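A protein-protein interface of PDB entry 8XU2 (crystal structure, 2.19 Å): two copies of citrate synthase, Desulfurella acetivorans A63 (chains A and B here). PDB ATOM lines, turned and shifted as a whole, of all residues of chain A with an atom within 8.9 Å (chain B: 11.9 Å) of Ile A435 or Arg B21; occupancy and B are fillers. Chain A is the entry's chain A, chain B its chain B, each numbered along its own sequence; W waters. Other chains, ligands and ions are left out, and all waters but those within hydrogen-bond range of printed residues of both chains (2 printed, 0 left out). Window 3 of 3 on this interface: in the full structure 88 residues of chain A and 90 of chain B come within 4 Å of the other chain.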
ATOM      1  N   ILE A  36      17.151 -19.555  -7.046  1.00  0.00           N
ATOM      2  CA  ILE A  36      17.444 -18.179  -6.692  1.00  0.00           C
ATOM      3  C   ILE A  36      16.182 -17.327  -6.871  1.00  0.00           C
ATOM      4  O   ILE A  36      15.852 -16.508  -6.020  1.00  0.00           O
ATOM      5  CB  ILE A  36      18.626 -17.640  -7.523  1.00  0.00           C
ATOM      6  CG1 ILE A  36      19.943 -18.293  -7.100  1.00  0.00           C
ATOM      7  CG2 ILE A  36      18.711 -16.120  -7.444  1.00  0.00           C
ATOM      8  CD1 ILE A  36      21.173 -17.728  -7.814  1.00  0.00           C
ATOM      9  N   ILE A  40      14.305 -15.165  -3.804  1.00  0.00           N
ATOM     10  CA  ILE A  40      14.075 -13.740  -3.964  1.00  0.00           C
ATOM     11  C   ILE A  40      12.577 -13.450  -4.126  1.00  0.00           C
ATOM     12  O   ILE A  40      12.109 -12.403  -3.687  1.00  0.00           O
ATOM     13  CB  ILE A  40      14.902 -13.196  -5.145  1.00  0.00           C
ATOM     14  CG1 ILE A  40      16.402 -13.207  -4.839  1.00  0.00           C
ATOM     15  CG2 ILE A  40      14.433 -11.811  -5.566  1.00  0.00           C
ATOM     16  CD1 ILE A  40      17.270 -12.795  -6.010  1.00  0.00           C
ATOM     17  N   THR A 426      22.457 -11.731  -0.354  1.00  0.00           N
ATOM     18  CA  THR A 426      22.653 -11.493  -1.775  1.00  0.00           C
ATOM     19  C   THR A 426      24.048 -11.973  -2.207  1.00  0.00           C
ATOM     20  O   THR A 426      24.188 -12.521  -3.298  1.00  0.00           O
ATOM     21  CB  THR A 426      22.400 -10.025  -2.139  1.00  0.00           C
ATOM     22  OG1 THR A 426      21.040  -9.695  -1.850  1.00  0.00           O
ATOM     23  CG2 THR A 426      22.633  -9.716  -3.601  1.00  0.00           C
ATOM     24  N   ASP A 427      25.065 -11.764  -1.358  1.00  0.00           N
ATOM     25  CA  ASP A 427      26.419 -12.248  -1.611  1.00  0.00           C
ATOM     26  C   ASP A 427      26.424 -13.758  -1.825  1.00  0.00           C
ATOM     27  O   ASP A 427      27.080 -14.247  -2.730  1.00  0.00           O
ATOM     28  CB  ASP A 427      27.376 -11.927  -0.453  1.00  0.00           C
ATOM     29  CG  ASP A 427      27.812 -10.480  -0.392  1.00  0.00           C
ATOM     30  OD1 ASP A 427      27.446  -9.713  -1.317  1.00  0.00           O
ATOM     31  OD2 ASP A 427      28.506 -10.137   0.583  1.00  0.00           O
ATOM     32  N   MET A 428      25.704 -14.484  -0.966  1.00  0.00           N
ATOM     33  CA  MET A 428      25.655 -15.928  -1.044  1.00  0.00           C
ATOM     34  C   MET A 428      24.966 -16.375  -2.332  1.00  0.00           C
ATOM     35  O   MET A 428      25.401 -17.342  -2.935  1.00  0.00           O
ATOM     36  CB  MET A 428      24.933 -16.509   0.169  1.00  0.00           C
ATOM     37  CG  MET A 428      25.779 -16.451   1.425  1.00  0.00           C
ATOM     38  SD  MET A 428      24.794 -16.706   2.915  1.00  0.00           S
ATOM     39  CE  MET A 428      24.541 -18.482   2.853  1.00  0.00           C
ATOM     40  N   LEU A 429      23.936 -15.642  -2.775  1.00  0.00           N
ATOM     41  CA  LEU A 429      23.258 -15.971  -4.021  1.00  0.00           C
ATOM     42  C   LEU A 429      24.192 -15.719  -5.206  1.00  0.00           C
ATOM     43  O   LEU A 429      24.151 -16.435  -6.205  1.00  0.00           O
ATOM     44  CB  LEU A 429      21.992 -15.122  -4.171  1.00  0.00           C
ATOM     45  CG  LEU A 429      20.870 -15.366  -3.159  1.00  0.00           C
ATOM     46  CD1 LEU A 429      19.749 -14.377  -3.388  1.00  0.00           C
ATOM     47  CD2 LEU A 429      20.328 -16.789  -3.230  1.00  0.00           C
ATOM     48  N   GLU A 430      24.967 -14.631  -5.111  1.00  0.00           N
ATOM     49  CA  GLU A 430      25.943 -14.278  -6.127  1.00  0.00           C
ATOM     50  C   GLU A 430      27.038 -15.342  -6.206  1.00  0.00           C
ATOM     51  O   GLU A 430      27.422 -15.737  -7.298  1.00  0.00           O
ATOM     52  CB  GLU A 430      26.460 -12.867  -5.844  1.00  0.00           C
ATOM     53  CG  GLU A 430      25.488 -11.807  -6.336  1.00  0.00           C
ATOM     54  CD  GLU A 430      25.898 -10.382  -6.036  1.00  0.00           C
ATOM     55  OE1 GLU A 430      26.788 -10.197  -5.207  1.00  0.00           O
ATOM     56  OE2 GLU A 430      25.320  -9.461  -6.644  1.00  0.00           O
ATOM     57  N   LYS A 431      27.502 -15.836  -5.057  1.00  0.00           N
ATOM     58  CA  LYS A 431      28.466 -16.927  -5.001  1.00  0.00           C
ATOM     59  C   LYS A 431      27.905 -18.141  -5.749  1.00  0.00           C
ATOM     60  O   LYS A 431      28.553 -18.659  -6.664  1.00  0.00           O
ATOM     61  CB  LYS A 431      28.812 -17.226  -3.537  1.00  0.00           C
ATOM     62  CG  LYS A 431      30.186 -17.833  -3.259  1.00  0.00           C
ATOM     63  CD  LYS A 431      30.452 -19.162  -3.933  1.00  0.00           C
ATOM     64  CE  LYS A 431      29.563 -20.299  -3.463  1.00  0.00           C
ATOM     65  NZ  LYS A 431      30.007 -20.843  -2.154  1.00  0.00           N
ATOM     66  N   TRP A 432      26.680 -18.574  -5.403  1.00  0.00           N
ATOM     67  CA  TRP A 432      26.084 -19.746  -6.029  1.00  0.00           C
ATOM     68  C   TRP A 432      25.849 -19.532  -7.521  1.00  0.00           C
ATOM     69  O   TRP A 432      25.828 -20.494  -8.273  1.00  0.00           O
ATOM     70  CB  TRP A 432      24.802 -20.174  -5.307  1.00  0.00           C
ATOM     71  CG  TRP A 432      25.081 -20.699  -3.929  1.00  0.00           C
ATOM     72  CD1 TRP A 432      26.144 -21.468  -3.552  1.00  0.00           C
ATOM     73  CD2 TRP A 432      24.307 -20.481  -2.732  1.00  0.00           C
ATOM     74  NE1 TRP A 432      26.096 -21.733  -2.208  1.00  0.00           N
ATOM     75  CE2 TRP A 432      24.974 -21.152  -1.679  1.00  0.00           C
ATOM     76  CE3 TRP A 432      23.138 -19.771  -2.441  1.00  0.00           C
ATOM     77  CZ2 TRP A 432      24.494 -21.153  -0.370  1.00  0.00           C
ATOM     78  CZ3 TRP A 432      22.667 -19.766  -1.143  1.00  0.00           C
ATOM     79  CH2 TRP A 432      23.331 -20.457  -0.127  1.00  0.00           C
ATOM     80  N   ALA A 433      25.635 -18.286  -7.940  1.00  0.00           N
ATOM     81  CA  ALA A 433      25.376 -17.967  -9.335  1.00  0.00           C
ATOM     82  C   ALA A 433      26.673 -17.936 -10.149  1.00  0.00           C
ATOM     83  O   ALA A 433      26.615 -17.880 -11.379  1.00  0.00           O
ATOM     84  CB  ALA A 433      24.658 -16.640  -9.436  1.00  0.00           C
ATOM     85  N   GLY A 434      27.825 -17.897  -9.456  1.00  0.00           N
ATOM     86  CA  GLY A 434      29.134 -17.815 -10.087  1.00  0.00           C
ATOM     87  C   GLY A 434      29.561 -16.388 -10.456  1.00  0.00           C
ATOM     88  O   GLY A 434      30.409 -16.189 -11.312  1.00  0.00           O
ATOM     89  N   ILE A 435      28.941 -15.380  -9.841  1.00  0.00           N
ATOM     90  CA  ILE A 435      29.333 -13.987 -10.031  1.00  0.00           C
ATOM     91  C   ILE A 435      30.499 -13.670  -9.094  1.00  0.00           C
ATOM     92  O   ILE A 435      30.524 -14.143  -7.959  1.00  0.00           O
ATOM     93  CB  ILE A 435      28.150 -13.039  -9.766  1.00  0.00           C
ATOM     94  CG1 ILE A 435      26.918 -13.397 -10.604  1.00  0.00           C
ATOM     95  CG2 ILE A 435      28.559 -11.587  -9.954  1.00  0.00           C
ATOM     96  CD1 ILE A 435      25.687 -12.572 -10.293  1.00  0.00           C
ATOM     97  N   LYS A 436      31.416 -12.808  -9.558  1.00  0.00           N
ATOM     98  CA  LYS A 436      32.773 -12.697  -9.036  1.00  0.00           C
ATOM     99  C   LYS A 436      32.794 -12.103  -7.619  1.00  0.00           C
ATOM    100  O   LYS A 436      33.108 -10.914  -7.511  1.00  0.00           O
ATOM    101  CB  LYS A 436      33.596 -11.841 -10.008  1.00  0.00           C
ATOM    102  N   ILE B  12      20.561   1.780  -1.972  1.00  0.00           N
ATOM    103  CA  ILE B  12      19.510   1.112  -2.723  1.00  0.00           C
ATOM    104  C   ILE B  12      19.846   1.164  -4.222  1.00  0.00           C
ATOM    105  O   ILE B  12      19.658   0.172  -4.921  1.00  0.00           O
ATOM    106  CB  ILE B  12      18.129   1.705  -2.384  1.00  0.00           C
ATOM    107  CG1 ILE B  12      17.714   1.348  -0.952  1.00  0.00           C
ATOM    108  CG2 ILE B  12      17.064   1.256  -3.388  1.00  0.00           C
ATOM    109  CD1 ILE B  12      16.617   2.237  -0.377  1.00  0.00           C
ATOM    110  N   ALA B  13      20.318   2.316  -4.714  1.00  0.00           N
ATOM    111  CA  ALA B  13      20.697   2.470  -6.113  1.00  0.00           C
ATOM    112  C   ALA B  13      21.789   1.463  -6.509  1.00  0.00           C
ATOM    113  O   ALA B  13      21.718   0.886  -7.594  1.00  0.00           O
ATOM    114  CB  ALA B  13      21.136   3.893  -6.376  1.00  0.00           C
ATOM    115  N   GLN B  14      22.760   1.222  -5.619  1.00  0.00           N
ATOM    116  CA  GLN B  14      23.836   0.269  -5.861  1.00  0.00           C
ATOM    117  C   GLN B  14      23.337  -1.175  -5.779  1.00  0.00           C
ATOM    118  O   GLN B  14      23.800  -2.031  -6.521  1.00  0.00           O
ATOM    119  CB  GLN B  14      24.977   0.468  -4.857  1.00  0.00           C
ATOM    120  CG  GLN B  14      25.877   1.646  -5.189  1.00  0.00           C
ATOM    121  CD  GLN B  14      26.304   2.459  -3.985  1.00  0.00           C
ATOM    122  OE1 GLN B  14      26.661   1.924  -2.933  1.00  0.00           O
ATOM    123  NE2 GLN B  14      26.251   3.780  -4.127  1.00  0.00           N
ATOM    124  N   HIS B  15      22.392  -1.459  -4.882  1.00  0.00           N
ATOM    125  CA  HIS B  15      22.015  -2.837  -4.631  1.00  0.00           C
ATOM    126  C   HIS B  15      21.024  -3.357  -5.675  1.00  0.00           C
ATOM    127  O   HIS B  15      21.100  -4.521  -6.048  1.00  0.00           O
ATOM    128  CB  HIS B  15      21.452  -2.988  -3.211  1.00  0.00           C
ATOM    129  CG  HIS B  15      21.357  -4.395  -2.706  1.00  0.00           C
ATOM    130  ND1 HIS B  15      20.547  -5.358  -3.270  1.00  0.00           N
ATOM    131  CD2 HIS B  15      21.996  -4.964  -1.645  1.00  0.00           C
ATOM    132  CE1 HIS B  15      20.684  -6.489  -2.577  1.00  0.00           C
ATOM    133  NE2 HIS B  15      21.572  -6.265  -1.563  1.00  0.00           N
ATOM    134  N   ARG B  16      20.088  -2.513  -6.125  1.00  0.00           N
ATOM    135  CA  ARG B  16      18.994  -2.975  -6.972  1.00  0.00           C
ATOM    136  C   ARG B  16      19.517  -3.728  -8.201  1.00  0.00           C
ATOM    137  O   ARG B  16      19.015  -4.813  -8.493  1.00  0.00           O
ATOM    138  CB  ARG B  16      18.038  -1.838  -7.363  1.00  0.00           C
ATOM    139  CG  ARG B  16      17.089  -1.458  -6.240  1.00  0.00           C
ATOM    140  CD  ARG B  16      15.684  -0.987  -6.638  1.00  0.00           C
ATOM    141  NE  ARG B  16      15.655   0.454  -6.761  1.00  0.00           N
ATOM    142  CZ  ARG B  16      14.806   1.291  -6.190  1.00  0.00           C
ATOM    143  NH1 ARG B  16      14.038   0.936  -5.177  1.00  0.00           N
ATOM    144  NH2 ARG B  16      14.746   2.530  -6.653  1.00  0.00           N
ATOM    145  N   PRO B  17      20.499  -3.194  -8.977  1.00  0.00           N
ATOM    146  CA  PRO B  17      21.004  -3.904 -10.162  1.00  0.00           C
ATOM    147  C   PRO B  17      21.466  -5.334  -9.883  1.00  0.00           C
ATOM    148  O   PRO B  17      21.258  -6.214 -10.715  1.00  0.00           O
ATOM    149  CB  PRO B  17      22.149  -3.016 -10.657  1.00  0.00           C
ATOM    150  CG  PRO B  17      21.747  -1.627 -10.185  1.00  0.00           C
ATOM    151  CD  PRO B  17      21.136  -1.869  -8.813  1.00  0.00           C
ATOM    152  N   ARG B  18      22.066  -5.566  -8.704  1.00  0.00           N
ATOM    153  CA  ARG B  18      22.495  -6.898  -8.299  1.00  0.00           C
ATOM    154  C   ARG B  18      21.319  -7.863  -8.197  1.00  0.00           C
ATOM    155  O   ARG B  18      21.423  -9.021  -8.618  1.00  0.00           O
ATOM    156  CB  ARG B  18      23.201  -6.837  -6.948  1.00  0.00           C
ATOM    157  CG  ARG B  18      24.460  -5.986  -6.937  1.00  0.00           C
ATOM    158  CD  ARG B  18      24.990  -5.826  -5.534  1.00  0.00           C
ATOM    159  NE  ARG B  18      25.339  -7.108  -4.937  1.00  0.00           N
ATOM    160  CZ  ARG B  18      25.556  -7.293  -3.638  1.00  0.00           C
ATOM    161  NH1 ARG B  18      25.409  -6.278  -2.795  1.00  0.00           N
ATOM    162  NH2 ARG B  18      25.832  -8.508  -3.192  1.00  0.00           N
ATOM    163  N   THR B  19      20.205  -7.384  -7.622  1.00  0.00           N
ATOM    164  CA  THR B  19      19.006  -8.195  -7.460  1.00  0.00           C
ATOM    165  C   THR B  19      18.396  -8.465  -8.839  1.00  0.00           C
ATOM    166  O   THR B  19      17.986  -9.592  -9.107  1.00  0.00           O
ATOM    167  CB  THR B  19      17.998  -7.535  -6.492  1.00  0.00           C
ATOM    168  OG1 THR B  19      18.606  -7.358  -5.206  1.00  0.00           O
ATOM    169  CG2 THR B  19      16.724  -8.344  -6.347  1.00  0.00           C
ATOM    170  N   THR B  20      18.335  -7.422  -9.685  1.00  0.00           N
ATOM    171  CA  THR B  20      17.818  -7.524 -11.045  1.00  0.00           C
ATOM    172  C   THR B  20      18.583  -8.586 -11.845  1.00  0.00           C
ATOM    173  O   THR B  20      17.979  -9.411 -12.535  1.00  0.00           O
ATOM    174  CB  THR B  20      17.893  -6.155 -11.737  1.00  0.00           C
ATOM    175  OG1 THR B  20      17.162  -5.256 -10.908  1.00  0.00           O
ATOM    176  CG2 THR B  20      17.329  -6.127 -13.143  1.00  0.00           C
ATOM    177  N   ARG B  21      19.916  -8.565 -11.722  1.00  0.00           N
ATOM    178  CA  ARG B  21      20.780  -9.479 -12.446  1.00  0.00           C
ATOM    179  C   ARG B  21      20.577 -10.921 -11.988  1.00  0.00           C
ATOM    180  O   ARG B  21      20.541 -11.831 -12.810  1.00  0.00           O
ATOM    181  CB  ARG B  21      22.242  -9.070 -12.271  1.00  0.00           C
ATOM    182  CG  ARG B  21      23.201  -9.932 -13.079  1.00  0.00           C
ATOM    183  CD  ARG B  21      24.607  -9.340 -13.034  1.00  0.00           C
ATOM    184  NE  ARG B  21      25.489 -10.073 -13.930  1.00  0.00           N
ATOM    185  CZ  ARG B  21      26.740 -10.415 -13.648  1.00  0.00           C
ATOM    186  NH1 ARG B  21      27.407  -9.751 -12.721  1.00  0.00           N
ATOM    187  NH2 ARG B  21      27.310 -11.414 -14.297  1.00  0.00           N
ATOM    188  N   LEU B  22      20.474 -11.149 -10.675  1.00  0.00           N
ATOM    189  CA  LEU B  22      20.253 -12.499 -10.171  1.00  0.00           C
ATOM    190  C   LEU B  22      18.952 -13.083 -10.729  1.00  0.00           C
ATOM    191  O   LEU B  22      18.887 -14.281 -11.033  1.00  0.00           O
ATOM    192  CB  LEU B  22      20.229 -12.476  -8.642  1.00  0.00           C
ATOM    193  CG  LEU B  22      21.570 -12.308  -7.956  1.00  0.00           C
ATOM    194  CD1 LEU B  22      21.379 -11.928  -6.489  1.00  0.00           C
ATOM    195  CD2 LEU B  22      22.354 -13.604  -8.080  1.00  0.00           C
ATOM    196  N   LEU B  23      17.916 -12.246 -10.858  1.00  0.00           N
ATOM    197  CA  LEU B  23      16.634 -12.705 -11.369  1.00  0.00           C
ATOM    198  C   LEU B  23      16.691 -12.870 -12.882  1.00  0.00           C
ATOM    199  O   LEU B  23      16.110 -13.813 -13.406  1.00  0.00           O
ATOM    200  CB  LEU B  23      15.529 -11.714 -10.980  1.00  0.00           C
ATOM    201  CG  LEU B  23      15.105 -11.730  -9.507  1.00  0.00           C
ATOM    202  CD1 LEU B  23      14.028 -10.687  -9.248  1.00  0.00           C
ATOM    203  CD2 LEU B  23      14.630 -13.126  -9.092  1.00  0.00           C
ATOM    204  N   LYS B  24      17.361 -11.947 -13.582  1.00  0.00           N
ATOM    205  CA  LYS B  24      17.338 -11.954 -15.040  1.00  0.00           C
ATOM    206  C   LYS B  24      18.182 -13.106 -15.591  1.00  0.00           C
ATOM    207  O   LYS B  24      17.721 -13.822 -16.476  1.00  0.00           O
ATOM    208  CB  LYS B  24      17.810 -10.635 -15.649  1.00  0.00           C
ATOM    209  CG  LYS B  24      17.491 -10.564 -17.130  1.00  0.00           C
ATOM    210  CD  LYS B  24      17.940  -9.320 -17.818  1.00  0.00           C
ATOM    211  CE  LYS B  24      17.648  -9.391 -19.309  1.00  0.00           C
ATOM    212  NZ  LYS B  24      17.413  -8.061 -19.935  1.00  0.00           N
ATOM    213  N   GLU B  25      19.404 -13.274 -15.065  1.00  0.00           N
ATOM    214  CA  GLU B  25      20.374 -14.197 -15.624  1.00  0.00           C
ATOM    215  C   GLU B  25      20.383 -15.542 -14.902  1.00  0.00           C
ATOM    216  O   GLU B  25      20.652 -16.549 -15.549  1.00  0.00           O
ATOM    217  CB  GLU B  25      21.784 -13.617 -15.546  1.00  0.00           C
ATOM    218  CG  GLU B  25      22.086 -12.509 -16.546  1.00  0.00           C
ATOM    219  CD  GLU B  25      23.555 -12.129 -16.550  1.00  0.00           C
ATOM    220  OE1 GLU B  25      24.392 -13.045 -16.696  1.00  0.00           O
ATOM    221  OE2 GLU B  25      23.855 -10.939 -16.405  1.00  0.00           O
ATOM    222  N   PHE B  26      20.158 -15.562 -13.574  1.00  0.00           N
ATOM    223  CA  PHE B  26      20.467 -16.735 -12.752  1.00  0.00           C
ATOM    224  C   PHE B  26      19.256 -17.226 -11.949  1.00  0.00           C
ATOM    225  O   PHE B  26      19.418 -17.961 -10.979  1.00  0.00           O
ATOM    226  CB  PHE B  26      21.646 -16.422 -11.825  1.00  0.00           C
ATOM    227  CG  PHE B  26      22.889 -15.999 -12.563  1.00  0.00           C
ATOM    228  CD1 PHE B  26      23.615 -16.935 -13.301  1.00  0.00           C
ATOM    229  CD2 PHE B  26      23.298 -14.667 -12.583  1.00  0.00           C
ATOM    230  CE1 PHE B  26      24.741 -16.549 -14.013  1.00  0.00           C
ATOM    231  CE2 PHE B  26      24.420 -14.287 -13.309  1.00  0.00           C
ATOM    232  CZ  PHE B  26      25.144 -15.229 -14.014  1.00  0.00           C
ATOM    233  N   GLY B  27      18.048 -16.862 -12.405  1.00  0.00           N
ATOM    234  CA  GLY B  27      16.807 -17.181 -11.721  1.00  0.00           C
ATOM    235  C   GLY B  27      16.651 -18.674 -11.428  1.00  0.00           C
ATOM    236  O   GLY B  27      16.114 -19.037 -10.391  1.00  0.00           O
ATOM    237  N   ASN B  28      17.146 -19.543 -12.332  1.00  0.00           N
ATOM    238  CA  ASN B  28      16.824 -20.964 -12.274  1.00  0.00           C
ATOM    239  C   ASN B  28      17.931 -21.768 -11.620  1.00  0.00           C
ATOM    240  O   ASN B  28      17.821 -22.991 -11.530  1.00  0.00           O
ATOM    241  CB  ASN B  28      16.448 -21.537 -13.640  1.00  0.00           C
ATOM    242  CG  ASN B  28      15.000 -21.222 -13.975  1.00  0.00           C
ATOM    243  OD1 ASN B  28      14.717 -20.469 -14.906  1.00  0.00           O
ATOM    244  ND2 ASN B  28      14.069 -21.744 -13.188  1.00  0.00           N
ATOM    245  N   VAL B  29      18.963 -21.095 -11.111  1.00  0.00           N
ATOM    246  CA  VAL B  29      20.016 -21.773 -10.368  1.00  0.00           C
ATOM    247  C   VAL B  29      19.429 -22.321  -9.072  1.00  0.00           C
ATOM    248  O   VAL B  29      18.834 -21.586  -8.279  1.00  0.00           O
ATOM    249  CB  VAL B  29      21.193 -20.814 -10.084  1.00  0.00           C
ATOM    250  CG1 VAL B  29      22.193 -21.403  -9.098  1.00  0.00           C
ATOM    251  CG2 VAL B  29      21.864 -20.341 -11.383  1.00  0.00           C
ATOM    252  N   ILE B  31      19.422 -23.692  -5.340  1.00  0.00           N
ATOM    253  CA  ILE B  31      20.197 -23.411  -4.137  1.00  0.00           C
ATOM    254  C   ILE B  31      19.856 -24.393  -3.019  1.00  0.00           C
ATOM    255  O   ILE B  31      20.595 -24.466  -2.046  1.00  0.00           O
ATOM    256  CB  ILE B  31      20.034 -21.945  -3.693  1.00  0.00           C
ATOM    257  CG1 ILE B  31      18.594 -21.616  -3.282  1.00  0.00           C
ATOM    258  CG2 ILE B  31      20.544 -21.004  -4.783  1.00  0.00           C
ATOM    259  CD1 ILE B  31      18.437 -20.250  -2.612  1.00  0.00           C
ATOM    260  N   LYS B 163       7.006   1.229  -7.440  1.00  0.00           N
ATOM    261  CA  LYS B 163       7.919   0.220  -6.920  1.00  0.00           C
ATOM    262  C   LYS B 163       9.295   0.824  -6.636  1.00  0.00           C
ATOM    263  O   LYS B 163      10.060   0.253  -5.879  1.00  0.00           O
ATOM    264  CB  LYS B 163       8.037  -0.971  -7.876  1.00  0.00           C
ATOM    265  CG  LYS B 163       8.892  -0.678  -9.098  1.00  0.00           C
ATOM    266  CD  LYS B 163       9.213  -1.848  -9.994  1.00  0.00           C
ATOM    267  CE  LYS B 163       9.911  -1.355 -11.249  1.00  0.00           C
ATOM    268  NZ  LYS B 163      10.678  -2.427 -11.918  1.00  0.00           N
ATOM    269  N   LEU B 414      13.863  -3.305  -2.604  1.00  0.00           N
ATOM    270  CA  LEU B 414      14.231  -4.317  -3.584  1.00  0.00           C
ATOM    271  C   LEU B 414      12.995  -4.956  -4.220  1.00  0.00           C
ATOM    272  O   LEU B 414      13.134  -5.834  -5.063  1.00  0.00           O
ATOM    273  CB  LEU B 414      15.100  -5.372  -2.893  1.00  0.00           C
ATOM    274  CG  LEU B 414      16.390  -4.840  -2.279  1.00  0.00           C
ATOM    275  CD1 LEU B 414      17.223  -5.964  -1.666  1.00  0.00           C
ATOM    276  CD2 LEU B 414      17.196  -4.060  -3.317  1.00  0.00           C
ATOM    277  N   TYR B 416      10.736  -7.065  -3.149  1.00  0.00           N
ATOM    278  CA  TYR B 416      10.510  -8.476  -2.873  1.00  0.00           C
ATOM    279  C   TYR B 416       9.020  -8.808  -2.932  1.00  0.00           C
ATOM    280  O   TYR B 416       8.173  -8.069  -2.432  1.00  0.00           O
ATOM    281  CB  TYR B 416      11.146  -8.879  -1.541  1.00  0.00           C
ATOM    282  CG  TYR B 416      12.655  -8.949  -1.529  1.00  0.00           C
ATOM    283  CD1 TYR B 416      13.401  -9.012  -2.701  1.00  0.00           C
ATOM    284  CD2 TYR B 416      13.338  -9.047  -0.339  1.00  0.00           C
ATOM    285  CE1 TYR B 416      14.778  -9.122  -2.676  1.00  0.00           C
ATOM    286  CE2 TYR B 416      14.716  -9.149  -0.288  1.00  0.00           C
ATOM    287  CZ  TYR B 416      15.442  -9.213  -1.468  1.00  0.00           C
ATOM    288  OH  TYR B 416      16.813  -9.348  -1.443  1.00  0.00           O
HETATM  289  O   HOH W   1      23.911  -9.836  -9.007  1.00  0.00           O
HETATM  290  O   HOH W   2      18.945  -9.200  -3.285  1.00  0.00           O
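Printed residues of chain A that touch a printed residue of chain B: Ile A36, Ile A40, Thr A426, Asp A427, Leu A429, Glu A430, Trp A432, Ala A433 and Ile A435.
Along chain A the printed residues that touch a printed residue of chain B span positions 36 to 435.
Hydrophobic or aromatic side chains of chain B that line the printed part of chain A: His B15, Leu B22, Leu B23, Phe B26, Val B29, Ile B31 and Tyr B416.
Among the printed residues, Asp or Glu carboxylates within 4 Å of a Lys or Arg side-chain nitrogen of the other chain: Asp A427 with Arg B18 (2.8 Å) and Glu A430 with Arg B18 (2.8 Å).
The backbone NH (N) of Ile A435 lies within hydrogen-bond range of the backbone carbonyl oxygen (O) of Glu A430 (3.0 Å).
ND1 of His B15 is in hydrogen-bond range of OG1 of Thr B19.
NE of Arg B21 is in salt-bridge range of OE2 of Glu B25 (3.1 Å).
N of Gly B27 sits at hydrogen-bond distance from O of Leu B22 (3.0 Å).
No position is printed for both chains.
Of the printed residues of chain B, Ile A36 touches Phe B26, Gly B27, Val B29 and Ile B31.
Of the printed residues of chain B, Leu A429 touches Leu B22 (3.8 Å) and Ile B31 (3.99 Å).
Of the printed residues of chain B, Ile A435 touches Arg B21 (3.5 Å) and Phe B26 (3.7 Å).
No residue of chain B comes within 4 Å of Lys A436.
Thr B20 touches none of the printed residues of chain A.
Arg B21 touches just one residue of chain A: Ile A435.
Of the printed residues of chain A, Val B29 touches Ile A36 (2.9 Å) and Trp A432 (3.8 Å).
Of the printed residues of chain A, Ile B31 touches Ile A36 (3.6 Å), Leu A429 (3.99 Å) and Trp A432 (3.7 Å).
Of the printed residues of chain A, Tyr B416 touches Ile A40.
The nearest residue of chain B that does not touch Ile A435 is Leu B22 (4.1 Å).
The nearest residue of chain A that does not touch Arg B21 is Lys A436 (6.0 Å).
The nearest printed residue of chain A that does not touch Tyr B416 is Thr A426 (4.3 Å).
Water W2 lies within hydrogen-bond range of OG1 of Thr A426, OG1 of Thr B19 and OH of Tyr B416.
Water W1 lies within hydrogen-bond range of the backbone carbonyl oxygen of Arg B18 (2.6 Å) and the side-chain carboxylate of Glu A430 (2.8 Å).
The backbone carbonyl oxygen (O) of Val B29 lies within hydrogen-bond range of the backbone NH (N) of Ile A36 (2.9 Å).
NE2 of His B15 lies close to OG1 of Thr A426 (3.5 Å).
OD1 of Asp A427 lies within salt-bridge range of NH2 of Arg B18 (2.8 Å).
The side-chain carboxylate of Glu A430 is in salt-bridge range of the guanidinium group of Arg B18 (2.8 Å).
Phe B26 touches Ile A36 (O to CB, 3.6 Å).
CG1 of Ile A36 touches CG2 of Ile B31, at 3.6 Å.
Ile A40 touches Leu B22 (CD1 to CB, 3.97 Å).
CG2 of Ile A40 touches CD2 of Leu B23, at 3.8 Å.
Thr A426 touches Leu B22.
Leu B22 touches Leu A429.
Ile B31 touches Leu A429.
Val B29 touches Trp A432.
CE3 of Trp A432 touches CG2 of Ile B31 (3.7 Å).
Arg B21 touches Ile A435 (NH1 to CG2, 3.5 Å).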
